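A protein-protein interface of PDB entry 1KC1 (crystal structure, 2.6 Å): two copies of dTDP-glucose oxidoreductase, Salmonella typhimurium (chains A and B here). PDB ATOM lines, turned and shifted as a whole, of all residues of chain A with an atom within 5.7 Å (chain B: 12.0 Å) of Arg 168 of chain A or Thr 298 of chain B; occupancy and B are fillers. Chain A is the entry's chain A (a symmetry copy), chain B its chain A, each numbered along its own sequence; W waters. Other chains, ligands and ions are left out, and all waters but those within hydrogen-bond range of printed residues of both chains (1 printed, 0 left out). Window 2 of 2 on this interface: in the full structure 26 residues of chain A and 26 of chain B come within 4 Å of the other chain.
NZ of Lys 164 of chain A sits at hydrogen-bond distance from O of Thr 297 of chain B (3.3 Å).
O of Met 293 of chain B lies within hydrogen-bond range of OG1 of Thr 296 of chain B.
The backbone carbonyl oxygen of Met 293 of chain A lies within hydrogen-bond range of the side-chain hydroxyl of Thr 296 of chain A, 2.7 Å away.
Among the printed residues, pairs that only touch across the chains: Lys 171 of chain A with Thr 298 of chain B, Thr 296 of chain A with Thr 296 of chain B and Arg 168 of chain A with Thr 298 of chain B.
No residue of chain B comes within 4 Å of Thr 165 of chain A.
No residue of chain B comes within 4 Å of Leu 167 of chain A.
Of the printed residues of chain B, Arg 168 of chain A touches Thr 298 (3.6 Å).
No residue of chain B comes within 4 Å of Leu 169 of chain A.
No residue of chain B comes within 4 Å of Ala 170 of chain A.
Lys 171 of chain A touches just one residue of chain B: Thr 298 (3.2 Å).
No residue of chain B comes within 4 Å of Glu 172 of chain A.
Thr 296 of chain A touches just one residue of chain B: Thr 296 (3.3 Å).
Glu 292 of chain B touches none of the printed residues of chain A.
Printed residues of chain A within 4 Å of Thr 296 of chain B: Thr 296.
Printed residues of chain A within 4 Å of Thr 297 of chain B: Lys 164.
Thr 298 of chain B touches just these residues of chain A: Arg 168 (3.6 Å) and Lys 171 (3.2 Å).
The nearest residue of chain A that does not touch Thr 298 of chain B is Thr 296 of chain A (4.4 Å).
Of the 14 printed residues of chain A, 4 touch a printed residue of chain B.
Printed residues of chain A that touch a printed residue of chain B: Lys 164, Arg 168, Lys 171 and Thr 296.
Of the 8 printed residues of chain B, 3 touch a printed residue of chain A.
Among the printed residues, no Asp or Glu carboxylate lies within 4 Å of a Lys or Arg side-chain nitrogen of the other chain.
Thr 296 of chain B touches its own counterpart, Thr 296 of chain A.
Positions printed for both chains: 293 and 296.
Of the 4 pairs that touch across the chains among the printed residues, 1 has its exchanged pair printed and touching as well.
Water W1 lies within hydrogen-bond range of the side-chain amino group of Lys 164 of chain A (2.8 Å) and the side-chain hydroxyl of Thr 297 of chain B (3.1 Å).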
ATOM      1  N   ASN A 160      33.200  -3.709  14.673  1.00  0.00           N
ATOM      2  CA  ASN A 160      33.829  -4.715  15.504  1.00  0.00           C
ATOM      3  C   ASN A 160      34.671  -4.098  16.580  1.00  0.00           C
ATOM      4  O   ASN A 160      35.286  -3.097  16.320  1.00  0.00           O
ATOM      5  CB  ASN A 160      34.698  -5.633  14.650  1.00  0.00           C
ATOM      6  CG  ASN A 160      34.715  -7.066  15.205  1.00  0.00           C
ATOM      7  OD1 ASN A 160      33.750  -7.465  15.874  1.00  0.00           O
ATOM      8  ND2 ASN A 160      35.808  -7.842  14.953  1.00  0.00           N
ATOM      9  N   ALA A 163      34.659  -5.896  23.388  1.00  0.00           N
ATOM     10  CA  ALA A 163      33.381  -6.104  24.066  1.00  0.00           C
ATOM     11  C   ALA A 163      32.381  -6.910  23.228  1.00  0.00           C
ATOM     12  O   ALA A 163      31.702  -7.835  23.704  1.00  0.00           O
ATOM     13  CB  ALA A 163      32.755  -4.738  24.386  1.00  0.00           C
ATOM     14  N   LYS A 164      32.241  -6.480  21.984  1.00  0.00           N
ATOM     15  CA  LYS A 164      31.325  -7.162  21.082  1.00  0.00           C
ATOM     16  C   LYS A 164      31.694  -8.620  20.928  1.00  0.00           C
ATOM     17  O   LYS A 164      30.885  -9.457  21.207  1.00  0.00           O
ATOM     18  CB  LYS A 164      31.274  -6.517  19.694  1.00  0.00           C
ATOM     19  CG  LYS A 164      30.023  -5.636  19.412  1.00  0.00           C
ATOM     20  CD  LYS A 164      29.964  -5.041  17.970  1.00  0.00           C
ATOM     21  CE  LYS A 164      29.395  -3.600  17.986  1.00  0.00           C
ATOM     22  NZ  LYS A 164      28.886  -3.163  16.638  1.00  0.00           N
ATOM     23  N   THR A 165      32.905  -8.914  20.461  1.00  0.00           N
ATOM     24  CA  THR A 165      33.283 -10.280  20.141  1.00  0.00           C
ATOM     25  C   THR A 165      33.124 -11.169  21.386  1.00  0.00           C
ATOM     26  O   THR A 165      32.747 -12.339  21.274  1.00  0.00           O
ATOM     27  CB  THR A 165      34.715 -10.356  19.519  1.00  0.00           C
ATOM     28  OG1 THR A 165      35.668  -9.875  20.459  1.00  0.00           O
ATOM     29  CG2 THR A 165      34.904  -9.392  18.326  1.00  0.00           C
ATOM     30  N   MET A 166      33.388 -10.601  22.561  1.00  0.00           N
ATOM     31  CA  MET A 166      33.212 -11.297  23.839  1.00  0.00           C
ATOM     32  C   MET A 166      31.733 -11.520  24.188  1.00  0.00           C
ATOM     33  O   MET A 166      31.345 -12.555  24.683  1.00  0.00           O
ATOM     34  CB  MET A 166      33.846 -10.472  24.954  1.00  0.00           C
ATOM     35  CG  MET A 166      35.389 -10.375  24.898  1.00  0.00           C
ATOM     36  SD  MET A 166      36.111 -12.026  24.911  1.00  0.00           S
ATOM     37  CE  MET A 166      37.247 -11.860  23.541  1.00  0.00           C
ATOM     38  N   LEU A 167      30.897 -10.531  23.976  1.00  0.00           N
ATOM     39  CA  LEU A 167      29.476 -10.712  24.262  1.00  0.00           C
ATOM     40  C   LEU A 167      28.912 -11.834  23.423  1.00  0.00           C
ATOM     41  O   LEU A 167      28.183 -12.686  23.931  1.00  0.00           O
ATOM     42  CB  LEU A 167      28.681  -9.446  23.975  1.00  0.00           C
ATOM     43  CG  LEU A 167      28.646  -8.502  25.163  1.00  0.00           C
ATOM     44  CD1 LEU A 167      27.937  -7.211  24.771  1.00  0.00           C
ATOM     45  CD2 LEU A 167      27.989  -9.110  26.349  1.00  0.00           C
ATOM     46  N   ARG A 168      29.255 -11.779  22.132  1.00  0.00           N
ATOM     47  CA  ARG A 168      28.861 -12.740  21.094  1.00  0.00           C
ATOM     48  C   ARG A 168      29.238 -14.176  21.499  1.00  0.00           C
ATOM     49  O   ARG A 168      28.526 -15.130  21.194  1.00  0.00           O
ATOM     50  CB  ARG A 168      29.562 -12.370  19.775  1.00  0.00           C
ATOM     51  CG  ARG A 168      28.816 -12.755  18.526  1.00  0.00           C
ATOM     52  CD  ARG A 168      29.587 -12.526  17.233  1.00  0.00           C
ATOM     53  NE  ARG A 168      29.109 -11.313  16.595  1.00  0.00           N
ATOM     54  CZ  ARG A 168      29.721 -10.140  16.668  1.00  0.00           C
ATOM     55  NH1 ARG A 168      30.870 -10.017  17.320  1.00  0.00           N
ATOM     56  NH2 ARG A 168      29.193  -9.082  16.068  1.00  0.00           N
ATOM     57  N   LEU A 169      30.383 -14.292  22.164  1.00  0.00           N
ATOM     58  CA  LEU A 169      30.845 -15.532  22.747  1.00  0.00           C
ATOM     59  C   LEU A 169      29.928 -15.843  23.940  1.00  0.00           C
ATOM     60  O   LEU A 169      29.321 -16.910  23.999  1.00  0.00           O
ATOM     61  CB  LEU A 169      32.325 -15.403  23.163  1.00  0.00           C
ATOM     62  CG  LEU A 169      33.422 -15.571  22.082  1.00  0.00           C
ATOM     63  CD1 LEU A 169      34.780 -15.261  22.660  1.00  0.00           C
ATOM     64  CD2 LEU A 169      33.460 -16.962  21.470  1.00  0.00           C
ATOM     65  N   ALA A 170      29.791 -14.887  24.853  1.00  0.00           N
ATOM     66  CA  ALA A 170      28.945 -15.015  26.042  1.00  0.00           C
ATOM     67  C   ALA A 170      27.467 -15.409  25.788  1.00  0.00           C
ATOM     68  O   ALA A 170      26.824 -15.920  26.697  1.00  0.00           O
ATOM     69  CB  ALA A 170      29.017 -13.721  26.853  1.00  0.00           C
ATOM     70  N   LYS A 171      26.931 -15.126  24.592  1.00  0.00           N
ATOM     71  CA  LYS A 171      25.553 -15.514  24.184  1.00  0.00           C
ATOM     72  C   LYS A 171      25.573 -17.001  23.694  1.00  0.00           C
ATOM     73  O   LYS A 171      24.779 -17.862  24.110  1.00  0.00           O
ATOM     74  CB  LYS A 171      24.986 -14.589  23.044  1.00  0.00           C
ATOM     75  CG  LYS A 171      24.805 -12.994  23.312  1.00  0.00           C
ATOM     76  CD  LYS A 171      24.068 -12.192  22.145  1.00  0.00           C
ATOM     77  CE  LYS A 171      23.665 -10.716  22.561  1.00  0.00           C
ATOM     78  NZ  LYS A 171      23.321  -9.694  21.456  1.00  0.00           N
ATOM     79  N   GLU A 172      26.525 -17.280  22.811  1.00  0.00           N
ATOM     80  CA  GLU A 172      26.743 -18.587  22.198  1.00  0.00           C
ATOM     81  C   GLU A 172      27.362 -19.623  23.184  1.00  0.00           C
ATOM     82  O   GLU A 172      27.090 -20.820  23.066  1.00  0.00           O
ATOM     83  CB  GLU A 172      27.626 -18.318  20.942  1.00  0.00           C
ATOM     84  CG  GLU A 172      28.526 -19.401  20.356  1.00  0.00           C
ATOM     85  CD  GLU A 172      29.652 -18.814  19.467  1.00  0.00           C
ATOM     86  OE1 GLU A 172      30.050 -17.643  19.678  1.00  0.00           O
ATOM     87  OE2 GLU A 172      30.159 -19.520  18.555  1.00  0.00           O
ATOM     88  N   ARG A 173      28.152 -19.174  24.174  1.00  0.00           N
ATOM     89  CA  ARG A 173      28.904 -20.091  25.082  1.00  0.00           C
ATOM     90  C   ARG A 173      28.620 -20.040  26.592  1.00  0.00           C
ATOM     91  O   ARG A 173      28.024 -19.093  27.122  1.00  0.00           O
ATOM     92  CB  ARG A 173      30.403 -19.882  24.905  1.00  0.00           C
ATOM     93  CG  ARG A 173      31.016 -20.720  23.826  1.00  0.00           C
ATOM     94  CD  ARG A 173      32.515 -20.889  23.972  1.00  0.00           C
ATOM     95  NE  ARG A 173      33.222 -20.472  22.769  1.00  0.00           N
ATOM     96  CZ  ARG A 173      34.522 -20.608  22.581  1.00  0.00           C
ATOM     97  NH1 ARG A 173      35.297 -21.149  23.509  1.00  0.00           N
ATOM     98  NH2 ARG A 173      35.061 -20.168  21.460  1.00  0.00           N
ATOM     99  N   MET A 293      25.267   0.543  22.364  1.00  0.00           N
ATOM    100  CA  MET A 293      25.135  -0.778  21.728  1.00  0.00           C
ATOM    101  C   MET A 293      23.893  -1.524  22.117  1.00  0.00           C
ATOM    102  O   MET A 293      23.316  -2.182  21.290  1.00  0.00           O
ATOM    103  CB  MET A 293      26.337  -1.692  22.055  1.00  0.00           C
ATOM    104  CG  MET A 293      27.662  -1.353  21.279  1.00  0.00           C
ATOM    105  SD  MET A 293      28.969  -2.664  21.525  1.00  0.00           S
ATOM    106  CE  MET A 293      27.929  -4.120  21.694  1.00  0.00           C
ATOM    107  N   THR A 296      19.405  -0.543  21.179  1.00  0.00           N
ATOM    108  CA  THR A 296      19.175  -0.654  19.739  1.00  0.00           C
ATOM    109  C   THR A 296      17.668  -0.600  19.353  1.00  0.00           C
ATOM    110  O   THR A 296      16.924  -1.607  19.433  1.00  0.00           O
ATOM    111  CB  THR A 296      19.826  -1.930  19.121  1.00  0.00           C
ATOM    112  OG1 THR A 296      20.962  -2.379  19.889  1.00  0.00           O
ATOM    113  CG2 THR A 296      20.410  -1.574  17.751  1.00  0.00           C
ATOM    114  N   THR B 291      23.629   7.087   8.468  1.00  0.00           N
ATOM    115  CA  THR B 291      24.585   5.983   8.270  1.00  0.00           C
ATOM    116  C   THR B 291      24.823   5.215   9.577  1.00  0.00           C
ATOM    117  O   THR B 291      24.854   4.011   9.534  1.00  0.00           O
ATOM    118  CB  THR B 291      25.895   6.469   7.669  1.00  0.00           C
ATOM    119  OG1 THR B 291      25.684   7.064   6.370  1.00  0.00           O
ATOM    120  CG2 THR B 291      26.797   5.321   7.417  1.00  0.00           C
ATOM    121  N   GLU B 292      24.943   5.873  10.739  1.00  0.00           N
ATOM    122  CA  GLU B 292      24.995   5.139  12.051  1.00  0.00           C
ATOM    123  C   GLU B 292      23.669   4.358  12.314  1.00  0.00           C
ATOM    124  O   GLU B 292      23.659   3.300  12.879  1.00  0.00           O
ATOM    125  CB  GLU B 292      25.365   6.050  13.238  1.00  0.00           C
ATOM    126  CG  GLU B 292      26.693   6.763  13.083  1.00  0.00           C
ATOM    127  CD  GLU B 292      27.123   7.477  14.318  1.00  0.00           C
ATOM    128  OE1 GLU B 292      26.264   8.115  14.900  1.00  0.00           O
ATOM    129  OE2 GLU B 292      28.305   7.410  14.747  1.00  0.00           O
ATOM    130  N   MET B 293      22.553   4.872  11.869  1.00  0.00           N
ATOM    131  CA  MET B 293      21.256   4.199  12.052  1.00  0.00           C
ATOM    132  C   MET B 293      21.082   2.968  11.214  1.00  0.00           C
ATOM    133  O   MET B 293      20.506   2.016  11.675  1.00  0.00           O
ATOM    134  CB  MET B 293      20.074   5.141  11.731  1.00  0.00           C
ATOM    135  CG  MET B 293      19.767   6.223  12.830  1.00  0.00           C
ATOM    136  SD  MET B 293      18.168   7.127  12.491  1.00  0.00           S
ATOM    137  CE  MET B 293      17.228   5.818  11.694  1.00  0.00           C
ATOM    138  N   PHE B 294      21.574   3.011   9.981  1.00  0.00           N
ATOM    139  CA  PHE B 294      21.450   1.912   9.004  1.00  0.00           C
ATOM    140  C   PHE B 294      22.479   0.821   9.088  1.00  0.00           C
ATOM    141  O   PHE B 294      22.310  -0.207   8.504  1.00  0.00           O
ATOM    142  CB  PHE B 294      21.650   2.499   7.627  1.00  0.00           C
ATOM    143  CG  PHE B 294      20.596   3.448   7.212  1.00  0.00           C
ATOM    144  CD1 PHE B 294      19.330   3.417   7.770  1.00  0.00           C
ATOM    145  CD2 PHE B 294      20.861   4.358   6.240  1.00  0.00           C
ATOM    146  CE1 PHE B 294      18.391   4.265   7.351  1.00  0.00           C
ATOM    147  CE2 PHE B 294      19.884   5.181   5.803  1.00  0.00           C
ATOM    148  CZ  PHE B 294      18.660   5.133   6.348  1.00  0.00           C
ATOM    149  N   THR B 295      23.599   1.111   9.720  1.00  0.00           N
ATOM    150  CA  THR B 295      24.664   0.162   9.925  1.00  0.00           C
ATOM    151  C   THR B 295      24.444  -0.450  11.305  1.00  0.00           C
ATOM    152  O   THR B 295      25.234  -0.295  12.224  1.00  0.00           O
ATOM    153  CB  THR B 295      26.021   0.890   9.809  1.00  0.00           C
ATOM    154  OG1 THR B 295      26.243   1.216   8.423  1.00  0.00           O
ATOM    155  CG2 THR B 295      27.220  -0.012  10.213  1.00  0.00           C
ATOM    156  N   THR B 296      23.328  -1.142  11.441  1.00  0.00           N
ATOM    157  CA  THR B 296      23.006  -1.801  12.706  1.00  0.00           C
ATOM    158  C   THR B 296      23.494  -3.277  12.769  1.00  0.00           C
ATOM    159  O   THR B 296      22.845  -4.216  12.246  1.00  0.00           O
ATOM    160  CB  THR B 296      21.485  -1.739  13.048  1.00  0.00           C
ATOM    161  OG1 THR B 296      20.843  -0.600  12.437  1.00  0.00           O
ATOM    162  CG2 THR B 296      21.325  -1.503  14.552  1.00  0.00           C
ATOM    163  N   THR B 297      24.656  -3.456  13.397  1.00  0.00           N
ATOM    164  CA  THR B 297      25.156  -4.791  13.705  1.00  0.00           C
ATOM    165  C   THR B 297      25.321  -4.963  15.245  1.00  0.00           C
ATOM    166  O   THR B 297      25.722  -4.014  15.974  1.00  0.00           O
ATOM    167  CB  THR B 297      26.497  -5.135  12.939  1.00  0.00           C
ATOM    168  OG1 THR B 297      26.812  -4.137  11.949  1.00  0.00           O
ATOM    169  CG2 THR B 297      26.358  -6.459  12.143  1.00  0.00           C
ATOM    170  N   THR B 298      24.981  -6.186  15.695  1.00  0.00           N
ATOM    171  CA  THR B 298      25.108  -6.664  17.083  1.00  0.00           C
ATOM    172  C   THR B 298      25.969  -7.940  17.145  1.00  0.00           C
ATOM    173  O   THR B 298      25.461  -9.067  17.055  1.00  0.00           O
ATOM    174  CB  THR B 298      23.709  -6.957  17.668  1.00  0.00           C
ATOM    175  OG1 THR B 298      22.973  -5.729  17.799  1.00  0.00           O
ATOM    176  CG2 THR B 298      23.793  -7.533  19.107  1.00  0.00           C
HETATM  177  O   HOH W   1      29.067  -4.222  14.028  1.00  0.00           O
